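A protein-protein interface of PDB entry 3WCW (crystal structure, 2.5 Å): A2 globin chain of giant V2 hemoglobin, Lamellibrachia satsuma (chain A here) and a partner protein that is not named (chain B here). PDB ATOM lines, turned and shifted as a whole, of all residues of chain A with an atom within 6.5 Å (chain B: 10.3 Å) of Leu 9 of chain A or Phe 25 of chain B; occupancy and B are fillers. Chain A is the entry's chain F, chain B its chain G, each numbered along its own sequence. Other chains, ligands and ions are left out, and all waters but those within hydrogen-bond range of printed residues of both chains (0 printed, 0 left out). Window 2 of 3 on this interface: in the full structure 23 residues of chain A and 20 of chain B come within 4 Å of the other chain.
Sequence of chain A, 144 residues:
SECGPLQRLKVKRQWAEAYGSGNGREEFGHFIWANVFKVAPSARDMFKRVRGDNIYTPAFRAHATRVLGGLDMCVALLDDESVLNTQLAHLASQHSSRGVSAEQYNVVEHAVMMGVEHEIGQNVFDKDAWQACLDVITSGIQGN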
ATOM      1  N   GLY A   4      34.186 -33.578 -28.724  1.00  0.00           N
ATOM      2  CA  GLY A   4      33.861 -34.803 -28.024  1.00  0.00           C
ATOM      3  C   GLY A   4      33.400 -34.518 -26.610  1.00  0.00           C
ATOM      4  O   GLY A   4      33.255 -33.353 -26.230  1.00  0.00           O
ATOM      5  N   PRO A   5      33.146 -35.564 -25.807  1.00  0.00           N
ATOM      6  CA  PRO A   5      32.692 -35.422 -24.419  1.00  0.00           C
ATOM      7  C   PRO A   5      33.687 -34.661 -23.543  1.00  0.00           C
ATOM      8  O   PRO A   5      33.298 -33.832 -22.713  1.00  0.00           O
ATOM      9  CB  PRO A   5      32.509 -36.869 -23.972  1.00  0.00           C
ATOM     10  CG  PRO A   5      32.100 -37.544 -25.237  1.00  0.00           C
ATOM     11  CD  PRO A   5      33.086 -36.973 -26.223  1.00  0.00           C
ATOM     12  N   LEU A   6      34.970 -34.950 -23.730  1.00  0.00           N
ATOM     13  CA  LEU A   6      36.009 -34.278 -22.958  1.00  0.00           C
ATOM     14  C   LEU A   6      35.978 -32.774 -23.257  1.00  0.00           C
ATOM     15  O   LEU A   6      35.974 -31.960 -22.340  1.00  0.00           O
ATOM     16  CB  LEU A   6      37.385 -34.873 -23.295  1.00  0.00           C
ATOM     17  CG  LEU A   6      37.517 -36.397 -23.108  1.00  0.00           C
ATOM     18  CD1 LEU A   6      38.859 -36.877 -23.658  1.00  0.00           C
ATOM     19  CD2 LEU A   6      37.371 -36.760 -21.621  1.00  0.00           C
ATOM     20  N   GLN A   7      35.938 -32.405 -24.537  1.00  0.00           N
ATOM     21  CA  GLN A   7      35.910 -30.989 -24.913  1.00  0.00           C
ATOM     22  C   GLN A   7      34.703 -30.264 -24.321  1.00  0.00           C
ATOM     23  O   GLN A   7      34.805 -29.108 -23.913  1.00  0.00           O
ATOM     24  CB  GLN A   7      35.895 -30.830 -26.437  1.00  0.00           C
ATOM     25  CG  GLN A   7      37.191 -31.195 -27.142  1.00  0.00           C
ATOM     26  CD  GLN A   7      37.527 -32.669 -27.033  1.00  0.00           C
ATOM     27  OE1 GLN A   7      36.672 -33.533 -27.229  1.00  0.00           O
ATOM     28  NE2 GLN A   7      38.781 -32.964 -26.730  1.00  0.00           N
ATOM     29  N   ARG A   8      33.563 -30.952 -24.268  1.00  0.00           N
ATOM     30  CA  ARG A   8      32.342 -30.361 -23.728  1.00  0.00           C
ATOM     31  C   ARG A   8      32.466 -30.095 -22.233  1.00  0.00           C
ATOM     32  O   ARG A   8      31.979 -29.077 -21.744  1.00  0.00           O
ATOM     33  CB  ARG A   8      31.138 -31.269 -24.020  1.00  0.00           C
ATOM     34  CG  ARG A   8      30.788 -31.351 -25.520  1.00  0.00           C
ATOM     35  CD  ARG A   8      30.067 -32.642 -25.891  1.00  0.00           C
ATOM     36  NE  ARG A   8      29.953 -32.780 -27.346  1.00  0.00           N
ATOM     37  CZ  ARG A   8      28.940 -32.319 -28.079  1.00  0.00           C
ATOM     38  NH1 ARG A   8      27.923 -31.691 -27.495  1.00  0.00           N
ATOM     39  NH2 ARG A   8      28.975 -32.446 -29.405  1.00  0.00           N
ATOM     40  N   LEU A   9      33.116 -30.993 -21.499  1.00  0.00           N
ATOM     41  CA  LEU A   9      33.287 -30.765 -20.067  1.00  0.00           C
ATOM     42  C   LEU A   9      34.224 -29.576 -19.921  1.00  0.00           C
ATOM     43  O   LEU A   9      33.962 -28.660 -19.150  1.00  0.00           O
ATOM     44  CB  LEU A   9      33.908 -31.984 -19.370  1.00  0.00           C
ATOM     45  CG  LEU A   9      33.071 -33.263 -19.296  1.00  0.00           C
ATOM     46  CD1 LEU A   9      33.913 -34.379 -18.686  1.00  0.00           C
ATOM     47  CD2 LEU A   9      31.816 -33.016 -18.467  1.00  0.00           C
ATOM     48  N   LYS A  10      35.310 -29.603 -20.688  1.00  0.00           N
ATOM     49  CA  LYS A  10      36.316 -28.556 -20.665  1.00  0.00           C
ATOM     50  C   LYS A  10      35.664 -27.213 -20.901  1.00  0.00           C
ATOM     51  O   LYS A  10      35.913 -26.253 -20.174  1.00  0.00           O
ATOM     52  CB  LYS A  10      37.346 -28.795 -21.762  1.00  0.00           C
ATOM     53  CG  LYS A  10      38.482 -27.802 -21.794  1.00  0.00           C
ATOM     54  CD  LYS A  10      39.649 -28.265 -20.923  1.00  0.00           C
ATOM     55  CE  LYS A  10      40.916 -27.532 -21.309  1.00  0.00           C
ATOM     56  NZ  LYS A  10      42.141 -28.271 -20.934  1.00  0.00           N
ATOM     57  N   VAL A  11      34.833 -27.161 -21.941  1.00  0.00           N
ATOM     58  CA  VAL A  11      34.141 -25.949 -22.314  1.00  0.00           C
ATOM     59  C   VAL A  11      33.165 -25.568 -21.217  1.00  0.00           C
ATOM     60  O   VAL A  11      33.059 -24.388 -20.860  1.00  0.00           O
ATOM     61  CB  VAL A  11      33.429 -26.124 -23.688  1.00  0.00           C
ATOM     62  CG1 VAL A  11      32.308 -25.126 -23.841  1.00  0.00           C
ATOM     63  CG2 VAL A  11      34.433 -25.909 -24.813  1.00  0.00           C
ATOM     64  N   LYS A  12      32.464 -26.555 -20.668  1.00  0.00           N
ATOM     65  CA  LYS A  12      31.520 -26.280 -19.583  1.00  0.00           C
ATOM     66  C   LYS A  12      32.268 -25.676 -18.395  1.00  0.00           C
ATOM     67  O   LYS A  12      31.757 -24.781 -17.709  1.00  0.00           O
ATOM     68  CB  LYS A  12      30.817 -27.567 -19.135  1.00  0.00           C
ATOM     69  CG  LYS A  12      29.626 -27.981 -19.983  1.00  0.00           C
ATOM     70  CD  LYS A  12      29.393 -29.490 -19.850  1.00  0.00           C
ATOM     71  CE  LYS A  12      28.000 -29.901 -20.296  1.00  0.00           C
ATOM     72  NZ  LYS A  12      26.949 -29.370 -19.384  1.00  0.00           N
ATOM     73  N   ARG A  13      33.485 -26.160 -18.157  1.00  0.00           N
ATOM     74  CA  ARG A  13      34.287 -25.662 -17.047  1.00  0.00           C
ATOM     75  C   ARG A  13      34.853 -24.266 -17.304  1.00  0.00           C
ATOM     76  O   ARG A  13      34.788 -23.406 -16.430  1.00  0.00           O
ATOM     77  CB  ARG A  13      35.427 -26.633 -16.731  1.00  0.00           C
ATOM     78  CG  ARG A  13      36.101 -26.364 -15.386  1.00  0.00           C
ATOM     79  CD  ARG A  13      37.003 -27.518 -14.968  1.00  0.00           C
ATOM     80  NE  ARG A  13      38.047 -27.816 -15.955  1.00  0.00           N
ATOM     81  CZ  ARG A  13      39.022 -26.980 -16.298  1.00  0.00           C
ATOM     82  NH1 ARG A  13      39.927 -27.342 -17.204  1.00  0.00           N
ATOM     83  NH2 ARG A  13      39.091 -25.781 -15.737  1.00  0.00           N
ATOM     84  N   GLN A  14      35.399 -24.028 -18.493  1.00  0.00           N
ATOM     85  CA  GLN A  14      35.960 -22.717 -18.777  1.00  0.00           C
ATOM     86  C   GLN A  14      34.874 -21.676 -18.889  1.00  0.00           C
ATOM     87  O   GLN A  14      35.048 -20.537 -18.455  1.00  0.00           O
ATOM     88  CB  GLN A  14      36.814 -22.750 -20.032  1.00  0.00           C
ATOM     89  CG  GLN A  14      37.967 -23.714 -19.890  1.00  0.00           C
ATOM     90  CD  GLN A  14      39.100 -23.404 -20.826  1.00  0.00           C
ATOM     91  OE1 GLN A  14      38.876 -23.020 -21.968  1.00  0.00           O
ATOM     92  NE2 GLN A  14      40.336 -23.579 -20.353  1.00  0.00           N
ATOM     93  N   VAL A  75      25.856 -24.402 -23.674  1.00  0.00           N
ATOM     94  CA  VAL A  75      26.995 -24.970 -22.967  1.00  0.00           C
ATOM     95  C   VAL A  75      26.512 -25.936 -21.893  1.00  0.00           C
ATOM     96  O   VAL A  75      26.951 -27.087 -21.834  1.00  0.00           O
ATOM     97  CB  VAL A  75      27.854 -23.857 -22.328  1.00  0.00           C
ATOM     98  CG1 VAL A  75      28.879 -24.452 -21.364  1.00  0.00           C
ATOM     99  CG2 VAL A  75      28.545 -23.066 -23.431  1.00  0.00           C
ATOM    100  N   ALA A  76      25.592 -25.469 -21.058  1.00  0.00           N
ATOM    101  CA  ALA A  76      25.056 -26.293 -19.982  1.00  0.00           C
ATOM    102  C   ALA A  76      24.496 -27.605 -20.515  1.00  0.00           C
ATOM    103  O   ALA A  76      24.533 -28.622 -19.822  1.00  0.00           O
ATOM    104  CB  ALA A  76      23.966 -25.527 -19.236  1.00  0.00           C
ATOM    105  N   LEU A  77      23.992 -27.578 -21.752  1.00  0.00           N
ATOM    106  CA  LEU A  77      23.402 -28.764 -22.367  1.00  0.00           C
ATOM    107  C   LEU A  77      24.301 -29.590 -23.287  1.00  0.00           C
ATOM    108  O   LEU A  77      23.849 -30.596 -23.825  1.00  0.00           O
ATOM    109  CB  LEU A  77      22.135 -28.369 -23.125  1.00  0.00           C
ATOM    110  CG  LEU A  77      21.032 -27.781 -22.246  1.00  0.00           C
ATOM    111  CD1 LEU A  77      19.949 -27.111 -23.103  1.00  0.00           C
ATOM    112  CD2 LEU A  77      20.464 -28.899 -21.391  1.00  0.00           C
ATOM    113  N   LEU A  78      25.561 -29.194 -23.466  1.00  0.00           N
ATOM    114  CA  LEU A  78      26.471 -29.955 -24.334  1.00  0.00           C
ATOM    115  C   LEU A  78      26.514 -31.456 -24.018  1.00  0.00           C
ATOM    116  O   LEU A  78      26.818 -32.275 -24.888  1.00  0.00           O
ATOM    117  CB  LEU A  78      27.889 -29.391 -24.260  1.00  0.00           C
ATOM    118  CG  LEU A  78      28.020 -27.963 -24.787  1.00  0.00           C
ATOM    119  CD1 LEU A  78      29.427 -27.459 -24.533  1.00  0.00           C
ATOM    120  CD2 LEU A  78      27.682 -27.927 -26.279  1.00  0.00           C
ATOM    121  N   ASP A  79      26.201 -31.824 -22.783  1.00  0.00           N
ATOM    122  CA  ASP A  79      26.223 -33.235 -22.410  1.00  0.00           C
ATOM    123  C   ASP A  79      24.841 -33.868 -22.540  1.00  0.00           C
ATOM    124  O   ASP A  79      24.642 -35.013 -22.149  1.00  0.00           O
ATOM    125  CB  ASP A  79      26.731 -33.407 -20.969  1.00  0.00           C
ATOM    126  CG  ASP A  79      25.806 -32.779 -19.942  1.00  0.00           C
ATOM    127  OD1 ASP A  79      25.967 -33.075 -18.739  1.00  0.00           O
ATOM    128  OD2 ASP A  79      24.921 -31.985 -20.330  1.00  0.00           O
ATOM    129  N   VAL B  20      22.036 -22.440  -5.349  1.00  0.00           N
ATOM    130  CA  VAL B  20      21.081 -23.343  -5.977  1.00  0.00           C
ATOM    131  C   VAL B  20      21.371 -23.501  -7.477  1.00  0.00           C
ATOM    132  O   VAL B  20      21.108 -24.554  -8.057  1.00  0.00           O
ATOM    133  CB  VAL B  20      19.632 -22.829  -5.821  1.00  0.00           C
ATOM    134  CG1 VAL B  20      18.685 -23.750  -6.546  1.00  0.00           C
ATOM    135  CG2 VAL B  20      19.244 -22.757  -4.356  1.00  0.00           C
ATOM    136  N   TRP B  21      21.926 -22.459  -8.093  1.00  0.00           N
ATOM    137  CA  TRP B  21      22.212 -22.463  -9.530  1.00  0.00           C
ATOM    138  C   TRP B  21      23.455 -23.236  -9.985  1.00  0.00           C
ATOM    139  O   TRP B  21      24.591 -22.822  -9.746  1.00  0.00           O
ATOM    140  CB  TRP B  21      22.276 -21.013 -10.028  1.00  0.00           C
ATOM    141  CG  TRP B  21      22.827 -20.826 -11.414  1.00  0.00           C
ATOM    142  CD1 TRP B  21      24.147 -20.764 -11.776  1.00  0.00           C
ATOM    143  CD2 TRP B  21      22.075 -20.640 -12.620  1.00  0.00           C
ATOM    144  NE1 TRP B  21      24.261 -20.543 -13.132  1.00  0.00           N
ATOM    145  CE2 TRP B  21      23.005 -20.465 -13.674  1.00  0.00           C
ATOM    146  CE3 TRP B  21      20.708 -20.604 -12.915  1.00  0.00           C
ATOM    147  CZ2 TRP B  21      22.609 -20.257 -14.994  1.00  0.00           C
ATOM    148  CZ3 TRP B  21      20.315 -20.397 -14.232  1.00  0.00           C
ATOM    149  CH2 TRP B  21      21.262 -20.226 -15.252  1.00  0.00           C
ATOM    150  N   SER B  22      23.220 -24.360 -10.657  1.00  0.00           N
ATOM    151  CA  SER B  22      24.303 -25.198 -11.172  1.00  0.00           C
ATOM    152  C   SER B  22      24.911 -24.465 -12.375  1.00  0.00           C
ATOM    153  O   SER B  22      24.258 -24.299 -13.409  1.00  0.00           O
ATOM    154  CB  SER B  22      23.749 -26.573 -11.592  1.00  0.00           C
ATOM    155  OG  SER B  22      24.789 -27.497 -11.888  1.00  0.00           O
ATOM    156  N   ALA B  23      26.161 -24.026 -12.233  1.00  0.00           N
ATOM    157  CA  ALA B  23      26.838 -23.277 -13.289  1.00  0.00           C
ATOM    158  C   ALA B  23      27.282 -24.066 -14.529  1.00  0.00           C
ATOM    159  O   ALA B  23      27.323 -23.509 -15.635  1.00  0.00           O
ATOM    160  CB  ALA B  23      28.035 -22.536 -12.699  1.00  0.00           C
ATOM    161  N   GLN B  24      27.598 -25.350 -14.354  1.00  0.00           N
ATOM    162  CA  GLN B  24      28.065 -26.190 -15.463  1.00  0.00           C
ATOM    163  C   GLN B  24      27.054 -27.153 -16.096  1.00  0.00           C
ATOM    164  O   GLN B  24      27.182 -27.510 -17.271  1.00  0.00           O
ATOM    165  CB  GLN B  24      29.284 -27.001 -15.016  1.00  0.00           C
ATOM    166  CG  GLN B  24      30.543 -26.178 -14.806  1.00  0.00           C
ATOM    167  CD  GLN B  24      31.771 -27.037 -14.559  1.00  0.00           C
ATOM    168  OE1 GLN B  24      32.083 -27.936 -15.342  1.00  0.00           O
ATOM    169  NE2 GLN B  24      32.478 -26.759 -13.469  1.00  0.00           N
ATOM    170  N   PHE B  25      26.065 -27.582 -15.317  1.00  0.00           N
ATOM    171  CA  PHE B  25      25.067 -28.533 -15.800  1.00  0.00           C
ATOM    172  C   PHE B  25      23.636 -28.134 -15.483  1.00  0.00           C
ATOM    173  O   PHE B  25      23.324 -27.672 -14.388  1.00  0.00           O
ATOM    174  CB  PHE B  25      25.330 -29.918 -15.202  1.00  0.00           C
ATOM    175  CG  PHE B  25      26.623 -30.535 -15.641  1.00  0.00           C
ATOM    176  CD1 PHE B  25      26.776 -31.012 -16.936  1.00  0.00           C
ATOM    177  CD2 PHE B  25      27.688 -30.655 -14.752  1.00  0.00           C
ATOM    178  CE1 PHE B  25      27.976 -31.605 -17.343  1.00  0.00           C
ATOM    179  CE2 PHE B  25      28.890 -31.245 -15.146  1.00  0.00           C
ATOM    180  CZ  PHE B  25      29.034 -31.721 -16.443  1.00  0.00           C
ATOM    181  N   THR B  26      22.765 -28.346 -16.458  1.00  0.00           N
ATOM    182  CA  THR B  26      21.353 -28.029 -16.321  1.00  0.00           C
ATOM    183  C   THR B  26      20.696 -28.955 -15.305  1.00  0.00           C
ATOM    184  O   THR B  26      19.549 -28.741 -14.912  1.00  0.00           O
ATOM    185  CB  THR B  26      20.634 -28.204 -17.664  1.00  0.00           C
ATOM    186  OG1 THR B  26      20.590 -29.596 -18.008  1.00  0.00           O
ATOM    187  CG2 THR B  26      21.382 -27.450 -18.755  1.00  0.00           C
ATOM    188  N   GLY B  27      21.434 -29.979 -14.888  1.00  0.00           N
ATOM    189  CA  GLY B  27      20.923 -30.947 -13.932  1.00  0.00           C
ATOM    190  C   GLY B  27      20.114 -30.408 -12.763  1.00  0.00           C
ATOM    191  O   GLY B  27      19.003 -30.876 -12.510  1.00  0.00           O
ATOM    192  N   ARG B  28      20.667 -29.435 -12.047  1.00  0.00           N
ATOM    193  CA  ARG B  28      19.987 -28.849 -10.904  1.00  0.00           C
ATOM    194  C   ARG B  28      18.936 -27.810 -11.319  1.00  0.00           C
ATOM    195  O   ARG B  28      17.875 -27.715 -10.704  1.00  0.00           O
ATOM    196  CB  ARG B  28      21.029 -28.234  -9.956  1.00  0.00           C
ATOM    197  CG  ARG B  28      20.452 -27.515  -8.754  1.00  0.00           C
ATOM    198  CD  ARG B  28      21.389 -27.552  -7.543  1.00  0.00           C
ATOM    199  NE  ARG B  28      22.719 -27.026  -7.828  1.00  0.00           N
ATOM    200  CZ  ARG B  28      23.763 -27.772  -8.179  1.00  0.00           C
ATOM    201  NH1 ARG B  28      24.944 -27.204  -8.421  1.00  0.00           N
ATOM    202  NH2 ARG B  28      23.635 -29.091  -8.279  1.00  0.00           N
ATOM    203  N   ARG B  29      19.224 -27.039 -12.366  1.00  0.00           N
ATOM    204  CA  ARG B  29      18.285 -26.018 -12.854  1.00  0.00           C
ATOM    205  C   ARG B  29      16.950 -26.646 -13.247  1.00  0.00           C
ATOM    206  O   ARG B  29      15.879 -26.101 -12.969  1.00  0.00           O
ATOM    207  CB  ARG B  29      18.821 -25.318 -14.101  1.00  0.00           C
ATOM    208  CG  ARG B  29      20.231 -24.829 -14.042  1.00  0.00           C
ATOM    209  CD  ARG B  29      20.592 -24.235 -15.395  1.00  0.00           C
ATOM    210  NE  ARG B  29      21.997 -23.868 -15.482  1.00  0.00           N
ATOM    211  CZ  ARG B  29      22.540 -23.225 -16.512  1.00  0.00           C
ATOM    212  NH1 ARG B  29      21.796 -22.874 -17.556  1.00  0.00           N
ATOM    213  NH2 ARG B  29      23.832 -22.918 -16.494  1.00  0.00           N
ATOM    214  N   LEU B  30      17.042 -27.795 -13.911  1.00  0.00           N
ATOM    215  CA  LEU B  30      15.889 -28.528 -14.404  1.00  0.00           C
ATOM    216  C   LEU B  30      15.010 -29.038 -13.291  1.00  0.00           C
ATOM    217  O   LEU B  30      13.827 -28.744 -13.247  1.00  0.00           O
ATOM    218  CB  LEU B  30      16.369 -29.697 -15.271  1.00  0.00           C
ATOM    219  CG  LEU B  30      15.577 -30.108 -16.513  1.00  0.00           C
ATOM    220  CD1 LEU B  30      15.143 -28.887 -17.312  1.00  0.00           C
ATOM    221  CD2 LEU B  30      16.464 -31.005 -17.359  1.00  0.00           C
ATOM    222  N   ALA B  31      15.595 -29.805 -12.388  1.00  0.00           N
ATOM    223  CA  ALA B  31      14.842 -30.365 -11.272  1.00  0.00           C
ATOM    224  C   ALA B  31      13.977 -29.305 -10.597  1.00  0.00           C
ATOM    225  O   ALA B  31      12.777 -29.507 -10.385  1.00  0.00           O
ATOM    226  CB  ALA B  31      15.788 -30.977 -10.267  1.00  0.00           C
ATOM    227  N   ILE B  32      14.587 -28.173 -10.269  1.00  0.00           N
ATOM    228  CA  ILE B  32      13.869 -27.090  -9.621  1.00  0.00           C
ATOM    229  C   ILE B  32      12.812 -26.472 -10.524  1.00  0.00           C
ATOM    230  O   ILE B  32      11.721 -26.116 -10.060  1.00  0.00           O
ATOM    231  CB  ILE B  32      14.852 -26.027  -9.129  1.00  0.00           C
ATOM    232  CG1 ILE B  32      15.591 -26.580  -7.907  1.00  0.00           C
ATOM    233  CG2 ILE B  32      14.119 -24.739  -8.778  1.00  0.00           C
ATOM    234  CD1 ILE B  32      16.952 -25.990  -7.699  1.00  0.00           C
ATOM    235  N   ILE B  69      14.476 -24.813 -18.871  1.00  0.00           N
ATOM    236  CA  ILE B  69      15.789 -24.187 -18.928  1.00  0.00           C
ATOM    237  C   ILE B  69      15.623 -22.760 -19.410  1.00  0.00           C
ATOM    238  O   ILE B  69      16.298 -21.859 -18.922  1.00  0.00           O
ATOM    239  CB  ILE B  69      16.722 -24.968 -19.860  1.00  0.00           C
ATOM    240  CG1 ILE B  69      17.128 -26.270 -19.166  1.00  0.00           C
ATOM    241  CG2 ILE B  69      17.924 -24.128 -20.248  1.00  0.00           C
ATOM    242  CD1 ILE B  69      17.959 -27.178 -20.029  1.00  0.00           C
ATOM    243  N   VAL B  72      14.217 -20.716 -16.390  1.00  0.00           N
ATOM    244  CA  VAL B  72      15.263 -20.505 -15.406  1.00  0.00           C
ATOM    245  C   VAL B  72      16.322 -19.510 -15.881  1.00  0.00           C
ATOM    246  O   VAL B  72      16.743 -18.648 -15.110  1.00  0.00           O
ATOM    247  CB  VAL B  72      15.893 -21.863 -15.006  1.00  0.00           C
ATOM    248  CG1 VAL B  72      17.311 -21.682 -14.511  1.00  0.00           C
ATOM    249  CG2 VAL B  72      15.053 -22.485 -13.921  1.00  0.00           C
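The backbone carbonyl oxygen (O) of Ser 22 of chain B is in hydrogen-bond range of the guanidinium group (NE) of Arg 29 of chain B, at 3.1 Å. The side-chain amino group (NZ) of Lys 12 of chain A lies within hydrogen-bond range of the backbone carbonyl oxygen (O) of Ala 76 of chain A, at 2.6 Å. NZ of Lys 12 of chain A is in salt-bridge range of OD2 of Asp 79 of chain A, at 3.4 Å. The side-chain hydroxyl of Ser 22 of chain B is in hydrogen-bond range of the backbone carbonyl oxygen of Phe 25 of chain B, at 2.9 Å. The side-chain amino group (NZ) of Lys 12 of chain A lies within hydrogen-bond range of the backbone carbonyl oxygen (O) of Val 75 of chain A, 3.3 Å away.
Of chain A, only Leu 9, Lys 12 and Asp 79 come within 4 Å of Phe 25 of chain B. Lys 12 of chain A touches just these residues of chain B: Gln 24 (2.8 Å) and Phe 25 (3.0 Å). Ala 76 of chain A touches three residues of chain B. Of the printed residues of chain A, Ile 69 of chain B touches Leu 77 (3.3 Å). Printed residues of chain A within 4 Å of Gln 24 of chain B: Lys 12, Arg 13 and Ala 76. The nearest residue of chain B that does not touch Leu 9 of chain A is Gln 24 of chain B (4.3 Å). The nearest residue of chain A that does not touch Phe 25 of chain B is Ala 76 of chain A (4.1 Å).
Leu 9 of chain A touches Phe 25 of chain B. Phe 25 of chain B touches Lys 12 of chain A. Arg 13 of chain A touches Gln 24 of chain B (CA to OE1, 3.6 Å). O of Gln 24 of chain B touches CA of Ala 76 of chain A (3.7 Å). Ala 76 of chain A touches Thr 26 of chain B. Ala 76 of chain A touches Arg 29 of chain B (CB to NH2, 3.8 Å). CD2 of Leu 77 of chain A touches CG2 of Thr 26 of chain B, at 3.1 Å. Ile 69 of chain B touches Leu 77 of chain A. Asp 79 of chain A touches Phe 25 of chain B.
Of the 15 printed residues of chain B, 5 touch a printed residue of chain A. Among the printed residues, 10 pairs touch across the chains.
The side-chain amino group of Lys 12 of chain A is in hydrogen-bond range of the backbone carbonyl oxygen of Gln 24 of chain B, at 2.8 Å.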
